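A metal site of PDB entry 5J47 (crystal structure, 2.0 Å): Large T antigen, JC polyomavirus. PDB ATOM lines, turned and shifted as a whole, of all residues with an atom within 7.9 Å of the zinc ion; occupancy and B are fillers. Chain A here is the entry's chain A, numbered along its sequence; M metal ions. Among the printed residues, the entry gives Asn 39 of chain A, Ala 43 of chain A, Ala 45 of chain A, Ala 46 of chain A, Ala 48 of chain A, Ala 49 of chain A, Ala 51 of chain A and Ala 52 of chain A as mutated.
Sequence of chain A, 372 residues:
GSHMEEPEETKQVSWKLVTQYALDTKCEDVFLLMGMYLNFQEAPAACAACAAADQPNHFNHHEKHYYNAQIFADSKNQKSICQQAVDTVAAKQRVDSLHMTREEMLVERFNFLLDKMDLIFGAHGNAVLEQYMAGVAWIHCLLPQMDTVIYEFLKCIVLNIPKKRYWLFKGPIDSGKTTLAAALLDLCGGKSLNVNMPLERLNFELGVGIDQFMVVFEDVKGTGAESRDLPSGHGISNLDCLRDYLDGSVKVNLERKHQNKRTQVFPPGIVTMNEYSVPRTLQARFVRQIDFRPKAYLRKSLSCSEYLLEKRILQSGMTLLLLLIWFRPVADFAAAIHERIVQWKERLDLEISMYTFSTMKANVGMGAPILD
Of the 20 residues printed, 4 come within 4 Å of the zinc ion.
A ring nitrogen (NE2) of His 62 sits at hydrogen-bond distance from the backbone carbonyl oxygen of Phe 40 (3.0 Å). A ring nitrogen (NE2) of His 62 is in hydrogen-bond range of the backbone carbonyl oxygen of Glu 42, at 2.7 Å. The side-chain sulfur (SG) of Cys 47 lies close to the backbone NH (N) of Ala 49 (3.6 Å).
ND1 of His 62 binds the zinc ion, 2.0 Å away. A ring nitrogen (NE2) of His 58 binds the zinc ion, at 2.1 Å. SG of Cys 50 binds the zinc ion (2.2 Å). The side-chain sulfur (SG) of Cys 47 is bound to the zinc ion (2.3 Å). The zinc ion has four donor atoms within binding distance.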
ATOM      1  N   ASN A  39      24.598  32.061   8.592  1.00  0.00           N
ATOM      2  CA  ASN A  39      23.986  32.154   7.262  1.00  0.00           C
ATOM      3  C   ASN A  39      23.461  30.810   6.699  1.00  0.00           C
ATOM      4  O   ASN A  39      22.935  30.774   5.588  1.00  0.00           O
ATOM      5  CB  ASN A  39      24.931  32.844   6.277  1.00  0.00           C
ATOM      6  CG  ASN A  39      24.997  34.333   6.454  1.00  0.00           C
ATOM      7  OD1 ASN A  39      24.143  34.940   7.114  1.00  0.00           O
ATOM      8  ND2 ASN A  39      25.995  34.970   5.873  1.00  0.00           N
ATOM      9  N   PHE A  40      23.560  29.721   7.484  1.00  0.00           N
ATOM     10  CA  PHE A  40      23.035  28.408   7.124  1.00  0.00           C
ATOM     11  C   PHE A  40      21.661  28.131   7.797  1.00  0.00           C
ATOM     12  O   PHE A  40      21.035  27.122   7.493  1.00  0.00           O
ATOM     13  CB  PHE A  40      24.042  27.276   7.462  1.00  0.00           C
ATOM     14  CG  PHE A  40      25.378  27.266   6.761  1.00  0.00           C
ATOM     15  CD1 PHE A  40      25.485  27.550   5.408  1.00  0.00           C
ATOM     16  CD2 PHE A  40      26.533  26.882   7.445  1.00  0.00           C
ATOM     17  CE1 PHE A  40      26.723  27.502   4.761  1.00  0.00           C
ATOM     18  CE2 PHE A  40      27.770  26.834   6.798  1.00  0.00           C
ATOM     19  CZ  PHE A  40      27.847  27.142   5.457  1.00  0.00           C
ATOM     20  N   GLU A  42      18.644  29.613   7.485  1.00  0.00           N
ATOM     21  CA  GLU A  42      17.462  29.735   6.621  1.00  0.00           C
ATOM     22  C   GLU A  42      17.300  28.502   5.722  1.00  0.00           C
ATOM     23  O   GLU A  42      18.299  27.823   5.454  1.00  0.00           O
ATOM     24  CB  GLU A  42      17.515  31.019   5.768  1.00  0.00           C
ATOM     25  CG  GLU A  42      17.347  32.306   6.571  1.00  0.00           C
ATOM     26  CD  GLU A  42      15.952  32.572   7.080  1.00  0.00           C
ATOM     27  OE1 GLU A  42      15.156  33.197   6.342  1.00  0.00           O
ATOM     28  OE2 GLU A  42      15.653  32.168   8.231  1.00  0.00           O
ATOM     29  N   ALA A  43      16.070  28.213   5.274  1.00  0.00           N
ATOM     30  CA  ALA A  43      15.755  27.070   4.421  1.00  0.00           C
ATOM     31  C   ALA A  43      16.576  27.047   3.126  1.00  0.00           C
ATOM     32  O   ALA A  43      16.559  28.033   2.371  1.00  0.00           O
ATOM     33  CB  ALA A  43      14.265  27.021   4.115  1.00  0.00           C
ATOM     34  N   PRO A  44      17.335  25.963   2.853  1.00  0.00           N
ATOM     35  CA  PRO A  44      18.167  25.938   1.628  1.00  0.00           C
ATOM     36  C   PRO A  44      17.379  25.910   0.313  1.00  0.00           C
ATOM     37  O   PRO A  44      17.927  26.342  -0.701  1.00  0.00           O
ATOM     38  CB  PRO A  44      19.058  24.706   1.803  1.00  0.00           C
ATOM     39  CG  PRO A  44      18.405  23.874   2.829  1.00  0.00           C
ATOM     40  CD  PRO A  44      17.503  24.730   3.652  1.00  0.00           C
ATOM     41  N   ALA A  45      16.111  25.445   0.327  1.00  0.00           N
ATOM     42  CA  ALA A  45      15.232  25.386  -0.851  1.00  0.00           C
ATOM     43  C   ALA A  45      14.882  26.785  -1.368  1.00  0.00           C
ATOM     44  O   ALA A  45      14.763  26.976  -2.581  1.00  0.00           O
ATOM     45  CB  ALA A  45      13.959  24.610  -0.528  1.00  0.00           C
ATOM     46  N   ALA A  46      14.730  27.758  -0.454  1.00  0.00           N
ATOM     47  CA  ALA A  46      14.420  29.153  -0.773  1.00  0.00           C
ATOM     48  C   ALA A  46      15.643  30.075  -0.586  1.00  0.00           C
ATOM     49  O   ALA A  46      15.491  31.291  -0.501  1.00  0.00           O
ATOM     50  CB  ALA A  46      13.253  29.622   0.097  1.00  0.00           C
ATOM     51  N   CYS A  47      16.861  29.486  -0.524  1.00  0.00           N
ATOM     52  CA  CYS A  47      18.099  30.256  -0.348  1.00  0.00           C
ATOM     53  C   CYS A  47      18.608  30.840  -1.672  1.00  0.00           C
ATOM     54  O   CYS A  47      18.971  30.084  -2.578  1.00  0.00           O
ATOM     55  CB  CYS A  47      19.170  29.433   0.361  1.00  0.00           C
ATOM     56  SG  CYS A  47      20.725  30.329   0.643  1.00  0.00           S
ATOM     57  N   ALA A  48      18.621  32.191  -1.767  1.00  0.00           N
ATOM     58  CA  ALA A  48      19.099  32.936  -2.936  1.00  0.00           C
ATOM     59  C   ALA A  48      20.602  32.731  -3.163  1.00  0.00           C
ATOM     60  O   ALA A  48      21.037  32.649  -4.314  1.00  0.00           O
ATOM     61  CB  ALA A  48      18.778  34.415  -2.782  1.00  0.00           C
ATOM     62  N   ALA A  49      21.401  32.628  -2.068  1.00  0.00           N
ATOM     63  CA  ALA A  49      22.845  32.381  -2.126  1.00  0.00           C
ATOM     64  C   ALA A  49      23.135  31.002  -2.743  1.00  0.00           C
ATOM     65  O   ALA A  49      24.066  30.862  -3.541  1.00  0.00           O
ATOM     66  CB  ALA A  49      23.465  32.494  -0.739  1.00  0.00           C
ATOM     67  N   CYS A  50      22.294  29.995  -2.420  1.00  0.00           N
ATOM     68  CA  CYS A  50      22.403  28.646  -2.983  1.00  0.00           C
ATOM     69  C   CYS A  50      22.015  28.640  -4.459  1.00  0.00           C
ATOM     70  O   CYS A  50      22.675  27.956  -5.255  1.00  0.00           O
ATOM     71  CB  CYS A  50      21.598  27.638  -2.175  1.00  0.00           C
ATOM     72  SG  CYS A  50      22.459  27.025  -0.706  1.00  0.00           S
ATOM     73  N   ALA A  51      20.976  29.426  -4.831  1.00  0.00           N
ATOM     74  CA  ALA A  51      20.508  29.565  -6.220  1.00  0.00           C
ATOM     75  C   ALA A  51      21.555  30.272  -7.092  1.00  0.00           C
ATOM     76  O   ALA A  51      21.748  29.884  -8.244  1.00  0.00           O
ATOM     77  CB  ALA A  51      19.181  30.310  -6.259  1.00  0.00           C
ATOM     78  N   ALA A  52      22.244  31.304  -6.534  1.00  0.00           N
ATOM     79  CA  ALA A  52      23.295  32.076  -7.225  1.00  0.00           C
ATOM     80  C   ALA A  52      24.549  31.224  -7.482  1.00  0.00           C
ATOM     81  O   ALA A  52      25.193  31.402  -8.518  1.00  0.00           O
ATOM     82  CB  ALA A  52      23.665  33.305  -6.399  1.00  0.00           C
ATOM     83  N   GLN A  55      29.445  31.238  -4.203  1.00  0.00           N
ATOM     84  CA  GLN A  55      30.261  31.112  -2.988  1.00  0.00           C
ATOM     85  C   GLN A  55      30.271  29.654  -2.513  1.00  0.00           C
ATOM     86  O   GLN A  55      29.380  29.262  -1.758  1.00  0.00           O
ATOM     87  CB  GLN A  55      29.731  32.046  -1.889  1.00  0.00           C
ATOM     88  CG  GLN A  55      30.652  33.219  -1.577  1.00  0.00           C
ATOM     89  CD  GLN A  55      30.452  33.745  -0.174  1.00  0.00           C
ATOM     90  OE1 GLN A  55      29.357  34.194   0.204  1.00  0.00           O
ATOM     91  NE2 GLN A  55      31.502  33.723   0.624  1.00  0.00           N
ATOM     92  N   HIS A  58      29.604  28.457   1.029  1.00  0.00           N
ATOM     93  CA  HIS A  58      28.201  28.523   1.417  1.00  0.00           C
ATOM     94  C   HIS A  58      27.362  27.409   0.760  1.00  0.00           C
ATOM     95  O   HIS A  58      26.807  26.584   1.487  1.00  0.00           O
ATOM     96  CB  HIS A  58      27.574  29.908   1.166  1.00  0.00           C
ATOM     97  CG  HIS A  58      26.107  29.917   1.457  1.00  0.00           C
ATOM     98  ND1 HIS A  58      25.633  30.148   2.745  1.00  0.00           N
ATOM     99  CD2 HIS A  58      25.068  29.617   0.655  1.00  0.00           C
ATOM    100  CE1 HIS A  58      24.313  30.030   2.662  1.00  0.00           C
ATOM    101  NE2 HIS A  58      23.932  29.703   1.427  1.00  0.00           N
ATOM    102  N   PHE A  59      27.224  27.423  -0.591  1.00  0.00           N
ATOM    103  CA  PHE A  59      26.353  26.512  -1.325  1.00  0.00           C
ATOM    104  C   PHE A  59      26.722  25.022  -1.231  1.00  0.00           C
ATOM    105  O   PHE A  59      25.845  24.180  -1.431  1.00  0.00           O
ATOM    106  CB  PHE A  59      26.162  26.945  -2.802  1.00  0.00           C
ATOM    107  CG  PHE A  59      27.271  26.661  -3.794  1.00  0.00           C
ATOM    108  CD1 PHE A  59      27.464  25.366  -4.288  1.00  0.00           C
ATOM    109  CD2 PHE A  59      28.057  27.680  -4.298  1.00  0.00           C
ATOM    110  CE1 PHE A  59      28.467  25.102  -5.222  1.00  0.00           C
ATOM    111  CE2 PHE A  59      29.048  27.425  -5.248  1.00  0.00           C
ATOM    112  CZ  PHE A  59      29.248  26.136  -5.703  1.00  0.00           C
ATOM    113  N   ASN A  60      28.001  24.684  -0.960  1.00  0.00           N
ATOM    114  CA  ASN A  60      28.387  23.277  -0.848  1.00  0.00           C
ATOM    115  C   ASN A  60      28.212  22.732   0.573  1.00  0.00           C
ATOM    116  O   ASN A  60      28.409  21.534   0.801  1.00  0.00           O
ATOM    117  CB  ASN A  60      29.814  23.050  -1.366  1.00  0.00           C
ATOM    118  CG  ASN A  60      29.927  22.962  -2.872  1.00  0.00           C
ATOM    119  OD1 ASN A  60      29.120  22.314  -3.556  1.00  0.00           O
ATOM    120  ND2 ASN A  60      30.951  23.596  -3.420  1.00  0.00           N
ATOM    121  N   HIS A  61      27.811  23.592   1.507  1.00  0.00           N
ATOM    122  CA  HIS A  61      27.692  23.232   2.914  1.00  0.00           C
ATOM    123  C   HIS A  61      26.324  23.509   3.541  1.00  0.00           C
ATOM    124  O   HIS A  61      26.021  22.905   4.580  1.00  0.00           O
ATOM    125  CB  HIS A  61      28.808  23.922   3.713  1.00  0.00           C
ATOM    126  CG  HIS A  61      30.177  23.602   3.191  1.00  0.00           C
ATOM    127  ND1 HIS A  61      30.850  22.455   3.572  1.00  0.00           N
ATOM    128  CD2 HIS A  61      30.924  24.267   2.274  1.00  0.00           C
ATOM    129  CE1 HIS A  61      31.993  22.461   2.896  1.00  0.00           C
ATOM    130  NE2 HIS A  61      32.081  23.534   2.108  1.00  0.00           N
ATOM    131  N   HIS A  62      25.501  24.388   2.916  1.00  0.00           N
ATOM    132  CA  HIS A  62      24.205  24.806   3.459  1.00  0.00           C
ATOM    133  C   HIS A  62      23.291  23.645   3.866  1.00  0.00           C
ATOM    134  O   HIS A  62      22.874  23.597   5.028  1.00  0.00           O
ATOM    135  CB  HIS A  62      23.461  25.773   2.514  1.00  0.00           C
ATOM    136  CG  HIS A  62      22.356  26.552   3.172  1.00  0.00           C
ATOM    137  ND1 HIS A  62      21.724  27.593   2.518  1.00  0.00           N
ATOM    138  CD2 HIS A  62      21.813  26.442   4.408  1.00  0.00           C
ATOM    139  CE1 HIS A  62      20.820  28.072   3.361  1.00  0.00           C
ATOM    140  NE2 HIS A  62      20.835  27.402   4.509  1.00  0.00           N
ATOM    141  N   GLU A  63      23.006  22.725   2.937  1.00  0.00           N
ATOM    142  CA  GLU A  63      22.144  21.571   3.187  1.00  0.00           C
ATOM    143  C   GLU A  63      22.646  20.685   4.337  1.00  0.00           C
ATOM    144  O   GLU A  63      21.844  20.282   5.177  1.00  0.00           O
ATOM    145  CB  GLU A  63      21.969  20.749   1.895  1.00  0.00           C
ATOM    146  CG  GLU A  63      20.750  19.836   1.908  1.00  0.00           C
ATOM    147  CD  GLU A  63      19.428  20.500   1.589  1.00  0.00           C
ATOM    148  OE1 GLU A  63      19.248  20.969   0.449  1.00  0.00           O
ATOM    149  OE2 GLU A  63      18.537  20.500   2.484  1.00  0.00           O
HETATM  150 ZN    ZN M   1      22.229  28.552   0.817  1.00  0.00          ZN
